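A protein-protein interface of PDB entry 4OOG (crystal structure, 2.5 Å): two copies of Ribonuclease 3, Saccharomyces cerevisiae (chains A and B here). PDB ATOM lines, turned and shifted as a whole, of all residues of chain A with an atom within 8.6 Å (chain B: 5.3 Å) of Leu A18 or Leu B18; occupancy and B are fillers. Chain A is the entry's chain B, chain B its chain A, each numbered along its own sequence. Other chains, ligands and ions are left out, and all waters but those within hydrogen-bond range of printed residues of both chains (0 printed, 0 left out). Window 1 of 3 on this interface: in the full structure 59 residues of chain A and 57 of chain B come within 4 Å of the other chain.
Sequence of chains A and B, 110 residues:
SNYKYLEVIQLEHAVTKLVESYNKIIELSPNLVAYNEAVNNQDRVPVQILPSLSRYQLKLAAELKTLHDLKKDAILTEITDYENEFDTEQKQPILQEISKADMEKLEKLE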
ATOM      1  N   LEU A  11       9.004  -9.089 -11.193  1.00  0.00           N
ATOM      2  CA  LEU A  11       9.724  -8.392 -10.139  1.00  0.00           C
ATOM      3  C   LEU A  11      10.005  -9.297  -8.950  1.00  0.00           C
ATOM      4  O   LEU A  11      11.148  -9.416  -8.510  1.00  0.00           O
ATOM      5  CB  LEU A  11       8.925  -7.178  -9.676  1.00  0.00           C
ATOM      6  CG  LEU A  11       9.407  -5.833 -10.205  1.00  0.00           C
ATOM      7  CD1 LEU A  11       8.434  -4.741  -9.794  1.00  0.00           C
ATOM      8  CD2 LEU A  11      10.806  -5.552  -9.683  1.00  0.00           C
ATOM      9  N   GLU A  12       8.954  -9.929  -8.431  1.00  0.00           N
ATOM     10  CA  GLU A  12       9.072 -10.790  -7.261  1.00  0.00           C
ATOM     11  C   GLU A  12      10.062 -11.919  -7.512  1.00  0.00           C
ATOM     12  O   GLU A  12      10.849 -12.279  -6.636  1.00  0.00           O
ATOM     13  CB  GLU A  12       7.708 -11.361  -6.870  1.00  0.00           C
ATOM     14  CG  GLU A  12       6.766 -10.356  -6.224  1.00  0.00           C
ATOM     15  CD  GLU A  12       5.545 -11.013  -5.602  1.00  0.00           C
ATOM     16  OE1 GLU A  12       4.858 -11.788  -6.302  1.00  0.00           O
ATOM     17  OE2 GLU A  12       5.278 -10.759  -4.408  1.00  0.00           O
ATOM     18  N   HIS A  13      10.017 -12.468  -8.720  1.00  0.00           N
ATOM     19  CA  HIS A  13      10.934 -13.526  -9.113  1.00  0.00           C
ATOM     20  C   HIS A  13      12.357 -12.980  -9.195  1.00  0.00           C
ATOM     21  O   HIS A  13      13.296 -13.607  -8.703  1.00  0.00           O
ATOM     22  CB  HIS A  13      10.508 -14.116 -10.457  1.00  0.00           C
ATOM     23  CG  HIS A  13      11.175 -15.414 -10.790  1.00  0.00           C
ATOM     24  ND1 HIS A  13      12.443 -15.736 -10.356  1.00  0.00           N
ATOM     25  CD2 HIS A  13      10.744 -16.475 -11.512  1.00  0.00           C
ATOM     26  CE1 HIS A  13      12.766 -16.938 -10.800  1.00  0.00           C
ATOM     27  NE2 HIS A  13      11.751 -17.408 -11.504  1.00  0.00           N
ATOM     28  N   ALA A  14      12.505 -11.811  -9.812  1.00  0.00           N
ATOM     29  CA  ALA A  14      13.812 -11.175  -9.961  1.00  0.00           C
ATOM     30  C   ALA A  14      14.468 -10.886  -8.614  1.00  0.00           C
ATOM     31  O   ALA A  14      15.647 -11.174  -8.421  1.00  0.00           O
ATOM     32  CB  ALA A  14      13.692  -9.898 -10.773  1.00  0.00           C
ATOM     33  N   VAL A  15      13.699 -10.315  -7.692  1.00  0.00           N
ATOM     34  CA  VAL A  15      14.190 -10.026  -6.348  1.00  0.00           C
ATOM     35  C   VAL A  15      14.630 -11.307  -5.643  1.00  0.00           C
ATOM     36  O   VAL A  15      15.653 -11.338  -4.958  1.00  0.00           O
ATOM     37  CB  VAL A  15      13.111  -9.330  -5.491  1.00  0.00           C
ATOM     38  CG1 VAL A  15      13.597  -9.146  -4.061  1.00  0.00           C
ATOM     39  CG2 VAL A  15      12.725  -7.992  -6.101  1.00  0.00           C
ATOM     40  N   THR A  16      13.849 -12.365  -5.826  1.00  0.00           N
ATOM     41  CA  THR A  16      14.149 -13.656  -5.224  1.00  0.00           C
ATOM     42  C   THR A  16      15.431 -14.252  -5.807  1.00  0.00           C
ATOM     43  O   THR A  16      16.278 -14.760  -5.070  1.00  0.00           O
ATOM     44  CB  THR A  16      12.972 -14.637  -5.401  1.00  0.00           C
ATOM     45  OG1 THR A  16      11.863 -14.196  -4.609  1.00  0.00           O
ATOM     46  CG2 THR A  16      13.362 -16.033  -4.965  1.00  0.00           C
ATOM     47  N   LYS A  17      15.577 -14.175  -7.127  1.00  0.00           N
ATOM     48  CA  LYS A  17      16.786 -14.650  -7.798  1.00  0.00           C
ATOM     49  C   LYS A  17      18.002 -13.832  -7.381  1.00  0.00           C
ATOM     50  O   LYS A  17      19.100 -14.366  -7.238  1.00  0.00           O
ATOM     51  CB  LYS A  17      16.625 -14.597  -9.317  1.00  0.00           C
ATOM     52  CG  LYS A  17      15.927 -15.803  -9.928  1.00  0.00           C
ATOM     53  CD  LYS A  17      16.931 -16.830 -10.432  1.00  0.00           C
ATOM     54  CE  LYS A  17      16.263 -17.863 -11.331  1.00  0.00           C
ATOM     55  NZ  LYS A  17      15.579 -17.232 -12.500  1.00  0.00           N
ATOM     56  N   LEU A  18      17.795 -12.533  -7.190  1.00  0.00           N
ATOM     57  CA  LEU A  18      18.857 -11.637  -6.751  1.00  0.00           C
ATOM     58  C   LEU A  18      19.436 -12.075  -5.411  1.00  0.00           C
ATOM     59  O   LEU A  18      20.651 -12.197  -5.260  1.00  0.00           O
ATOM     60  CB  LEU A  18      18.329 -10.210  -6.635  1.00  0.00           C
ATOM     61  CG  LEU A  18      19.308  -9.199  -6.040  1.00  0.00           C
ATOM     62  CD1 LEU A  18      20.480  -8.977  -6.979  1.00  0.00           C
ATOM     63  CD2 LEU A  18      18.603  -7.891  -5.736  1.00  0.00           C
ATOM     64  N   VAL A  19      18.552 -12.309  -4.446  1.00  0.00           N
ATOM     65  CA  VAL A  19      18.956 -12.718  -3.105  1.00  0.00           C
ATOM     66  C   VAL A  19      19.596 -14.101  -3.112  1.00  0.00           C
ATOM     67  O   VAL A  19      20.648 -14.310  -2.508  1.00  0.00           O
ATOM     68  CB  VAL A  19      17.760 -12.724  -2.137  1.00  0.00           C
ATOM     69  CG1 VAL A  19      18.187 -13.224  -0.766  1.00  0.00           C
ATOM     70  CG2 VAL A  19      17.152 -11.331  -2.039  1.00  0.00           C
ATOM     71  N   GLU A  20      18.956 -15.042  -3.797  1.00  0.00           N
ATOM     72  CA  GLU A  20      19.480 -16.400  -3.900  1.00  0.00           C
ATOM     73  C   GLU A  20      20.843 -16.421  -4.586  1.00  0.00           C
ATOM     74  O   GLU A  20      21.700 -17.241  -4.252  1.00  0.00           O
ATOM     75  CB  GLU A  20      18.488 -17.304  -4.639  1.00  0.00           C
ATOM     76  CG  GLU A  20      17.269 -17.700  -3.809  1.00  0.00           C
ATOM     77  CD  GLU A  20      16.084 -18.122  -4.664  1.00  0.00           C
ATOM     78  OE1 GLU A  20      16.103 -17.850  -5.886  1.00  0.00           O
ATOM     79  OE2 GLU A  20      15.129 -18.718  -4.115  1.00  0.00           O
ATOM     80  N   SER A  21      21.042 -15.511  -5.537  1.00  0.00           N
ATOM     81  CA  SER A  21      22.303 -15.430  -6.268  1.00  0.00           C
ATOM     82  C   SER A  21      23.440 -14.989  -5.362  1.00  0.00           C
ATOM     83  O   SER A  21      24.497 -15.617  -5.332  1.00  0.00           O
ATOM     84  CB  SER A  21      22.184 -14.470  -7.453  1.00  0.00           C
ATOM     85  OG  SER A  21      21.202 -14.922  -8.369  1.00  0.00           O
ATOM     86  N   TYR A  22      23.217 -13.909  -4.619  1.00  0.00           N
ATOM     87  CA  TYR A  22      24.233 -13.391  -3.713  1.00  0.00           C
ATOM     88  C   TYR A  22      24.614 -14.394  -2.627  1.00  0.00           C
ATOM     89  O   TYR A  22      25.786 -14.508  -2.269  1.00  0.00           O
ATOM     90  CB  TYR A  22      23.785 -12.074  -3.076  1.00  0.00           C
ATOM     91  CG  TYR A  22      24.830 -11.479  -2.158  1.00  0.00           C
ATOM     92  CD1 TYR A  22      26.017 -10.966  -2.664  1.00  0.00           C
ATOM     93  CD2 TYR A  22      24.632 -11.435  -0.785  1.00  0.00           C
ATOM     94  CE1 TYR A  22      26.978 -10.423  -1.829  1.00  0.00           C
ATOM     95  CE2 TYR A  22      25.585 -10.894   0.060  1.00  0.00           C
ATOM     96  CZ  TYR A  22      26.757 -10.389  -0.468  1.00  0.00           C
ATOM     97  OH  TYR A  22      27.711  -9.850   0.366  1.00  0.00           O
ATOM     98  N   ASN A  23      23.631 -15.121  -2.104  1.00  0.00           N
ATOM     99  CA  ASN A  23      23.908 -16.101  -1.062  1.00  0.00           C
ATOM    100  C   ASN A  23      24.802 -17.217  -1.571  1.00  0.00           C
ATOM    101  O   ASN A  23      25.713 -17.659  -0.873  1.00  0.00           O
ATOM    102  CB  ASN A  23      22.618 -16.696  -0.500  1.00  0.00           C
ATOM    103  CG  ASN A  23      21.847 -15.716   0.357  1.00  0.00           C
ATOM    104  OD1 ASN A  23      22.426 -14.820   0.973  1.00  0.00           O
ATOM    105  ND2 ASN A  23      20.530 -15.886   0.409  1.00  0.00           N
ATOM    106  N   LYS A  24      24.543 -17.670  -2.793  1.00  0.00           N
ATOM    107  CA  LYS A  24      25.312 -18.771  -3.356  1.00  0.00           C
ATOM    108  C   LYS A  24      26.728 -18.319  -3.691  1.00  0.00           C
ATOM    109  O   LYS A  24      27.663 -19.121  -3.672  1.00  0.00           O
ATOM    110  CB  LYS A  24      24.616 -19.368  -4.582  1.00  0.00           C
ATOM    111  CG  LYS A  24      25.247 -20.663  -5.081  1.00  0.00           C
ATOM    112  CD  LYS A  24      24.193 -21.678  -5.515  1.00  0.00           C
ATOM    113  CE  LYS A  24      23.632 -22.466  -4.330  1.00  0.00           C
ATOM    114  NZ  LYS A  24      24.547 -23.554  -3.858  1.00  0.00           N
ATOM    115  N   ILE A  25      26.884 -17.032  -3.984  1.00  0.00           N
ATOM    116  CA  ILE A  25      28.207 -16.454  -4.191  1.00  0.00           C
ATOM    117  C   ILE A  25      29.030 -16.553  -2.912  1.00  0.00           C
ATOM    118  O   ILE A  25      30.118 -17.123  -2.904  1.00  0.00           O
ATOM    119  CB  ILE A  25      28.125 -14.978  -4.621  1.00  0.00           C
ATOM    120  CG1 ILE A  25      27.530 -14.865  -6.024  1.00  0.00           C
ATOM    121  CG2 ILE A  25      29.503 -14.326  -4.580  1.00  0.00           C
ATOM    122  CD1 ILE A  25      27.386 -13.442  -6.505  1.00  0.00           C
ATOM    123  N   TYR A  56      35.033 -12.525 -16.203  1.00  0.00           N
ATOM    124  CA  TYR A  56      34.807 -11.585 -15.105  1.00  0.00           C
ATOM    125  C   TYR A  56      34.157 -12.171 -13.846  1.00  0.00           C
ATOM    126  O   TYR A  56      34.433 -11.707 -12.740  1.00  0.00           O
ATOM    127  CB  TYR A  56      33.992 -10.379 -15.589  1.00  0.00           C
ATOM    128  CG  TYR A  56      32.500 -10.624 -15.668  1.00  0.00           C
ATOM    129  CD1 TYR A  56      31.949 -11.343 -16.720  1.00  0.00           C
ATOM    130  CD2 TYR A  56      31.641 -10.132 -14.691  1.00  0.00           C
ATOM    131  CE1 TYR A  56      30.588 -11.570 -16.796  1.00  0.00           C
ATOM    132  CE2 TYR A  56      30.278 -10.353 -14.758  1.00  0.00           C
ATOM    133  CZ  TYR A  56      29.756 -11.073 -15.814  1.00  0.00           C
ATOM    134  OH  TYR A  56      28.400 -11.300 -15.891  1.00  0.00           O
ATOM    135  N   GLN A  57      33.302 -13.178 -14.013  1.00  0.00           N
ATOM    136  CA  GLN A  57      32.482 -13.678 -12.905  1.00  0.00           C
ATOM    137  C   GLN A  57      33.266 -14.118 -11.667  1.00  0.00           C
ATOM    138  O   GLN A  57      32.991 -13.652 -10.559  1.00  0.00           O
ATOM    139  CB  GLN A  57      31.568 -14.816 -13.363  1.00  0.00           C
ATOM    140  CG  GLN A  57      30.487 -14.399 -14.339  1.00  0.00           C
ATOM    141  CD  GLN A  57      30.841 -14.744 -15.766  1.00  0.00           C
ATOM    142  OE1 GLN A  57      32.015 -14.757 -16.140  1.00  0.00           O
ATOM    143  NE2 GLN A  57      29.829 -15.041 -16.571  1.00  0.00           N
ATOM    144  N   LEU A  60      34.685 -11.300  -9.782  1.00  0.00           N
ATOM    145  CA  LEU A  60      33.602 -10.559  -9.148  1.00  0.00           C
ATOM    146  C   LEU A  60      33.054 -11.304  -7.933  1.00  0.00           C
ATOM    147  O   LEU A  60      32.684 -10.689  -6.933  1.00  0.00           O
ATOM    148  CB  LEU A  60      32.487 -10.280 -10.159  1.00  0.00           C
ATOM    149  CG  LEU A  60      31.261  -9.520  -9.654  1.00  0.00           C
ATOM    150  CD1 LEU A  60      31.665  -8.297  -8.841  1.00  0.00           C
ATOM    151  CD2 LEU A  60      30.377  -9.115 -10.825  1.00  0.00           C
ATOM    152  N   ALA A  61      33.009 -12.628  -8.020  1.00  0.00           N
ATOM    153  CA  ALA A  61      32.553 -13.439  -6.899  1.00  0.00           C
ATOM    154  C   ALA A  61      33.565 -13.398  -5.758  1.00  0.00           C
ATOM    155  O   ALA A  61      33.192 -13.333  -4.585  1.00  0.00           O
ATOM    156  CB  ALA A  61      32.305 -14.871  -7.344  1.00  0.00           C
ATOM    157  N   LEU A  64      33.360 -10.011  -3.901  1.00  0.00           N
ATOM    158  CA  LEU A  64      32.165  -9.890  -3.079  1.00  0.00           C
ATOM    159  C   LEU A  64      32.310 -10.733  -1.821  1.00  0.00           C
ATOM    160  O   LEU A  64      31.812 -10.368  -0.757  1.00  0.00           O
ATOM    161  CB  LEU A  64      30.916 -10.297  -3.860  1.00  0.00           C
ATOM    162  CG  LEU A  64      30.414  -9.266  -4.871  1.00  0.00           C
ATOM    163  CD1 LEU A  64      29.128  -9.740  -5.522  1.00  0.00           C
ATOM    164  CD2 LEU A  64      30.210  -7.919  -4.196  1.00  0.00           C
ATOM    165  N   ILE A  75      24.805  -2.479   1.561  1.00  0.00           N
ATOM    166  CA  ILE A  75      23.489  -2.788   1.025  1.00  0.00           C
ATOM    167  C   ILE A  75      23.250  -4.294   1.002  1.00  0.00           C
ATOM    168  O   ILE A  75      22.165  -4.764   1.343  1.00  0.00           O
ATOM    169  CB  ILE A  75      23.335  -2.244  -0.412  1.00  0.00           C
ATOM    170  CG1 ILE A  75      24.156  -0.963  -0.600  1.00  0.00           C
ATOM    171  CG2 ILE A  75      21.869  -2.011  -0.745  1.00  0.00           C
ATOM    172  CD1 ILE A  75      23.631   0.233   0.169  1.00  0.00           C
ATOM    173  N   LEU A  76      24.279  -5.042   0.619  1.00  0.00           N
ATOM    174  CA  LEU A  76      24.179  -6.490   0.459  1.00  0.00           C
ATOM    175  C   LEU A  76      23.738  -7.214   1.729  1.00  0.00           C
ATOM    176  O   LEU A  76      22.916  -8.129   1.673  1.00  0.00           O
ATOM    177  CB  LEU A  76      25.510  -7.056  -0.032  1.00  0.00           C
ATOM    178  CG  LEU A  76      26.020  -6.423  -1.325  1.00  0.00           C
ATOM    179  CD1 LEU A  76      27.453  -6.848  -1.602  1.00  0.00           C
ATOM    180  CD2 LEU A  76      25.108  -6.791  -2.485  1.00  0.00           C
ATOM    181  N   ILE A  79      20.034  -6.537   2.302  1.00  0.00           N
ATOM    182  CA  ILE A  79      19.175  -7.209   1.336  1.00  0.00           C
ATOM    183  C   ILE A  79      18.925  -8.676   1.682  1.00  0.00           C
ATOM    184  O   ILE A  79      17.804  -9.168   1.556  1.00  0.00           O
ATOM    185  CB  ILE A  79      19.746  -7.084  -0.087  1.00  0.00           C
ATOM    186  CG1 ILE A  79      19.789  -5.613  -0.501  1.00  0.00           C
ATOM    187  CG2 ILE A  79      18.909  -7.877  -1.072  1.00  0.00           C
ATOM    188  CD1 ILE A  79      20.412  -5.373  -1.853  1.00  0.00           C
ATOM    189  N   THR A  80      19.964  -9.375   2.126  1.00  0.00           N
ATOM    190  CA  THR A  80      19.819 -10.784   2.476  1.00  0.00           C
ATOM    191  C   THR A  80      18.977 -10.973   3.733  1.00  0.00           C
ATOM    192  O   THR A  80      18.225 -11.940   3.846  1.00  0.00           O
ATOM    193  CB  THR A  80      21.181 -11.471   2.672  1.00  0.00           C
ATOM    194  OG1 THR A  80      21.981 -10.706   3.582  1.00  0.00           O
ATOM    195  CG2 THR A  80      21.906 -11.591   1.346  1.00  0.00           C
ATOM    196  N   HIS B  13      27.227 -18.832 -13.109  1.00  0.00           N
ATOM    197  CA  HIS B  13      25.781 -18.710 -13.263  1.00  0.00           C
ATOM    198  C   HIS B  13      25.173 -17.796 -12.203  1.00  0.00           C
ATOM    199  O   HIS B  13      24.229 -17.057 -12.475  1.00  0.00           O
ATOM    200  CB  HIS B  13      25.112 -20.085 -13.223  1.00  0.00           C
ATOM    201  CG  HIS B  13      23.615 -20.032 -13.266  1.00  0.00           C
ATOM    202  ND1 HIS B  13      22.827 -20.287 -12.165  1.00  0.00           N
ATOM    203  CD2 HIS B  13      22.761 -19.756 -14.281  1.00  0.00           C
ATOM    204  CE1 HIS B  13      21.553 -20.169 -12.498  1.00  0.00           C
ATOM    205  NE2 HIS B  13      21.486 -19.847 -13.777  1.00  0.00           N
ATOM    206  N   ALA B  14      25.723 -17.845 -10.995  1.00  0.00           N
ATOM    207  CA  ALA B  14      25.208 -17.039  -9.893  1.00  0.00           C
ATOM    208  C   ALA B  14      25.487 -15.554 -10.111  1.00  0.00           C
ATOM    209  O   ALA B  14      24.611 -14.715  -9.905  1.00  0.00           O
ATOM    210  CB  ALA B  14      25.795 -17.505  -8.570  1.00  0.00           C
ATOM    211  N   VAL B  15      26.712 -15.242 -10.526  1.00  0.00           N
ATOM    212  CA  VAL B  15      27.111 -13.864 -10.788  1.00  0.00           C
ATOM    213  C   VAL B  15      26.311 -13.290 -11.952  1.00  0.00           C
ATOM    214  O   VAL B  15      25.807 -12.168 -11.879  1.00  0.00           O
ATOM    215  CB  VAL B  15      28.620 -13.766 -11.093  1.00  0.00           C
ATOM    216  CG1 VAL B  15      28.972 -12.392 -11.625  1.00  0.00           C
ATOM    217  CG2 VAL B  15      29.429 -14.079  -9.845  1.00  0.00           C
ATOM    218  N   THR B  16      26.191 -14.075 -13.018  1.00  0.00           N
ATOM    219  CA  THR B  16      25.373 -13.707 -14.167  1.00  0.00           C
ATOM    220  C   THR B  16      23.938 -13.384 -13.751  1.00  0.00           C
ATOM    221  O   THR B  16      23.433 -12.297 -14.042  1.00  0.00           O
ATOM    222  CB  THR B  16      25.357 -14.829 -15.226  1.00  0.00           C
ATOM    223  OG1 THR B  16      26.663 -14.962 -15.805  1.00  0.00           O
ATOM    224  CG2 THR B  16      24.344 -14.518 -16.320  1.00  0.00           C
ATOM    225  N   LYS B  17      23.298 -14.323 -13.059  1.00  0.00           N
ATOM    226  CA  LYS B  17      21.918 -14.151 -12.606  1.00  0.00           C
ATOM    227  C   LYS B  17      21.778 -12.995 -11.622  1.00  0.00           C
ATOM    228  O   LYS B  17      20.739 -12.339 -11.568  1.00  0.00           O
ATOM    229  CB  LYS B  17      21.390 -15.442 -11.977  1.00  0.00           C
ATOM    230  CG  LYS B  17      20.797 -16.419 -12.978  1.00  0.00           C
ATOM    231  CD  LYS B  17      19.422 -15.963 -13.445  1.00  0.00           C
ATOM    232  CE  LYS B  17      18.909 -16.831 -14.584  1.00  0.00           C
ATOM    233  NZ  LYS B  17      19.673 -16.603 -15.842  1.00  0.00           N
ATOM    234  N   LEU B  18      22.830 -12.753 -10.849  1.00  0.00           N
ATOM    235  CA  LEU B  18      22.847 -11.646  -9.905  1.00  0.00           C
ATOM    236  C   LEU B  18      22.678 -10.316 -10.632  1.00  0.00           C
ATOM    237  O   LEU B  18      21.851  -9.489 -10.244  1.00  0.00           O
ATOM    238  CB  LEU B  18      24.159 -11.642  -9.121  1.00  0.00           C
ATOM    239  CG  LEU B  18      24.340 -10.538  -8.079  1.00  0.00           C
ATOM    240  CD1 LEU B  18      23.595 -10.876  -6.799  1.00  0.00           C
ATOM    241  CD2 LEU B  18      25.815 -10.301  -7.802  1.00  0.00           C
ATOM    242  N   VAL B  19      23.456 -10.127 -11.694  1.00  0.00           N
ATOM    243  CA  VAL B  19      23.448  -8.880 -12.454  1.00  0.00           C
ATOM    244  C   VAL B  19      22.141  -8.676 -13.216  1.00  0.00           C
ATOM    245  O   VAL B  19      21.551  -7.594 -13.171  1.00  0.00           O
ATOM    246  CB  VAL B  19      24.624  -8.825 -13.448  1.00  0.00           C
ATOM    247  CG1 VAL B  19      24.577  -7.537 -14.253  1.00  0.00           C
ATOM    248  CG2 VAL B  19      25.943  -8.943 -12.708  1.00  0.00           C
ATOM    249  N   GLU B  20      21.698  -9.718 -13.914  1.00  0.00           N
ATOM    250  CA  GLU B  20      20.425  -9.684 -14.626  1.00  0.00           C
ATOM    251  C   GLU B  20      19.273  -9.345 -13.692  1.00  0.00           C
ATOM    252  O   GLU B  20      18.355  -8.614 -14.064  1.00  0.00           O
ATOM    253  CB  GLU B  20      20.143 -11.029 -15.291  1.00  0.00           C
ATOM    254  CG  GLU B  20      21.099 -11.391 -16.405  1.00  0.00           C
ATOM    255  CD  GLU B  20      20.722 -12.692 -17.084  1.00  0.00           C
ATOM    256  OE1 GLU B  20      19.770 -13.358 -16.613  1.00  0.00           O
ATOM    257  OE2 GLU B  20      21.374 -13.045 -18.090  1.00  0.00           O
ATOM    258  N   SER B  21      19.325  -9.883 -12.478  1.00  0.00           N
ATOM    259  CA  SER B  21      18.262  -9.669 -11.508  1.00  0.00           C
ATOM    260  C   SER B  21      18.139  -8.203 -11.121  1.00  0.00           C
ATOM    261  O   SER B  21      17.035  -7.667 -11.058  1.00  0.00           O
ATOM    262  CB  SER B  21      18.474 -10.532 -10.264  1.00  0.00           C
ATOM    263  OG  SER B  21      18.393 -11.908 -10.588  1.00  0.00           O
ATOM    264  N   TYR B  22      19.268  -7.550 -10.868  1.00  0.00           N
ATOM    265  CA  TYR B  22      19.239  -6.148 -10.469  1.00  0.00           C
ATOM    266  C   TYR B  22      18.764  -5.254 -11.610  1.00  0.00           C
ATOM    267  O   TYR B  22      18.016  -4.301 -11.390  1.00  0.00           O
ATOM    268  CB  TYR B  22      20.604  -5.680  -9.960  1.00  0.00           C
ATOM    269  CG  TYR B  22      20.557  -4.304  -9.332  1.00  0.00           C
ATOM    270  CD1 TYR B  22      19.787  -4.065  -8.200  1.00  0.00           C
ATOM    271  CD2 TYR B  22      21.278  -3.245  -9.871  1.00  0.00           C
ATOM    272  CE1 TYR B  22      19.735  -2.809  -7.620  1.00  0.00           C
ATOM    273  CE2 TYR B  22      21.233  -1.984  -9.295  1.00  0.00           C
ATOM    274  CZ  TYR B  22      20.460  -1.773  -8.172  1.00  0.00           C
ATOM    275  OH  TYR B  22      20.410  -0.524  -7.594  1.00  0.00           O
ATOM    276  N   ILE B  25      15.022  -5.565 -11.901  1.00  0.00           N
ATOM    277  CA  ILE B  25      14.390  -4.846 -10.804  1.00  0.00           C
ATOM    278  C   ILE B  25      14.356  -3.347 -11.079  1.00  0.00           C
ATOM    279  O   ILE B  25      13.294  -2.726 -11.055  1.00  0.00           O
ATOM    280  CB  ILE B  25      15.119  -5.097  -9.475  1.00  0.00           C
ATOM    281  CG1 ILE B  25      14.915  -6.544  -9.026  1.00  0.00           C
ATOM    282  CG2 ILE B  25      14.619  -4.140  -8.404  1.00  0.00           C
ATOM    283  CD1 ILE B  25      15.732  -6.924  -7.813  1.00  0.00           C
ATOM    284  N   LEU B  64      15.154  -0.529  -3.673  1.00  0.00           N
ATOM    285  CA  LEU B  64      16.353  -0.586  -4.499  1.00  0.00           C
ATOM    286  C   LEU B  64      16.240   0.363  -5.690  1.00  0.00           C
ATOM    287  O   LEU B  64      17.222   0.984  -6.097  1.00  0.00           O
ATOM    288  CB  LEU B  64      16.625  -2.017  -4.966  1.00  0.00           C
ATOM    289  CG  LEU B  64      17.107  -2.973  -3.874  1.00  0.00           C
ATOM    290  CD1 LEU B  64      17.393  -4.351  -4.448  1.00  0.00           C
ATOM    291  CD2 LEU B  64      18.338  -2.412  -3.179  1.00  0.00           C
ATOM    292  N   ILE B  79      28.847  -3.347  -9.685  1.00  0.00           N
ATOM    293  CA  ILE B  79      28.617  -4.747 -10.024  1.00  0.00           C
ATOM    294  C   ILE B  79      28.118  -4.918 -11.457  1.00  0.00           C
ATOM    295  O   ILE B  79      28.560  -5.817 -12.174  1.00  0.00           O
ATOM    296  CB  ILE B  79      27.622  -5.397  -9.040  1.00  0.00           C
ATOM    297  CG1 ILE B  79      28.268  -5.541  -7.662  1.00  0.00           C
ATOM    298  CG2 ILE B  79      27.160  -6.753  -9.549  1.00  0.00           C
ATOM    299  CD1 ILE B  79      27.334  -6.077  -6.603  1.00  0.00           C
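The side-chain hydroxyl (OG1) of Thr B16 lies within hydrogen-bond range of the side-chain amide nitrogen (NE2) of Gln A57, 3.3 Å away.
OE1 of Glu B20 is in salt-bridge range of NZ of Lys B17. OG of Ser A21 lies within hydrogen-bond range of O of Lys A17, at 2.5 Å. The backbone carbonyl oxygen (O) of Lys B17 lies within hydrogen-bond range of the side-chain hydroxyl (OG) of Ser B21 (2.6 Å).
CB of Ser B21 touches O of Ala A14 (3.4 Å). Ile B25 touches Ala A14. CE of Lys B17 touches NZ of Lys A17, at 3.9 Å. Ser B21 touches Leu A18. OG of Ser A21 touches CB of Lys B17, at 3.7 Å. Ser A21 touches Leu B18. CD1 of Ile A25 touches CD2 of Leu B18, 3.7 Å away. CG2 of Val B15 touches O of Gln A57 (3.7 Å). CG1 of Val B15 touches CD2 of Leu A60, at 3.7 Å. Ala A61 touches Val B15.
Of the printed residues of chain B, Leu A60 touches Val B15 (3.7 Å) and Ile B79 (3.9998 Å). Printed residues of chain A within 4 Å of Val B15: Ile A25, Tyr A56, Gln A57, Leu A60 and Ala A61. Of the printed residues of chain A, Lys B17 touches Lys A17 and Ser A21. Leu B18 touches four residues of chain A. Of the printed residues of chain A, Ile B79 touches Leu A60 (3.9998 Å). The nearest printed residue of chain B that does not touch Gln A57 is His B13 (5.6 Å).
Hydrophobic or aromatic side chains of chain B within 4 Å of the printed part of chain A: Ala B14, Val B15, Leu B18, Ile B25 and Leu B64. Printed residues of chain A that touch a printed residue of chain B: Leu A11, Ala A14, Val A15, Lys A17, Leu A18, Ser A21, Tyr A22, Ile A25, Tyr A56, Gln A57, Leu A60, Ala A61 and Ile A79. Among the printed residues, no Asp or Glu carboxylate lies within 4 Å of a Lys or Arg side-chain nitrogen of the other chain.
Lys A17 touches Ser B21, and with the chains exchanged Ser A21 touches Lys B17. Leu A18 touches Ser B21, and with the chains exchanged Ser A21 touches Leu B18. Tyr A22 touches Leu B18, but with the chains exchanged Leu A18 does not touch Tyr B22 (4.3 Å). Ile A79 touches Leu B64, but with the chains exchanged Leu A64 does not touch Ile B79 (4.2 Å). 13 positions are printed for both chains.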
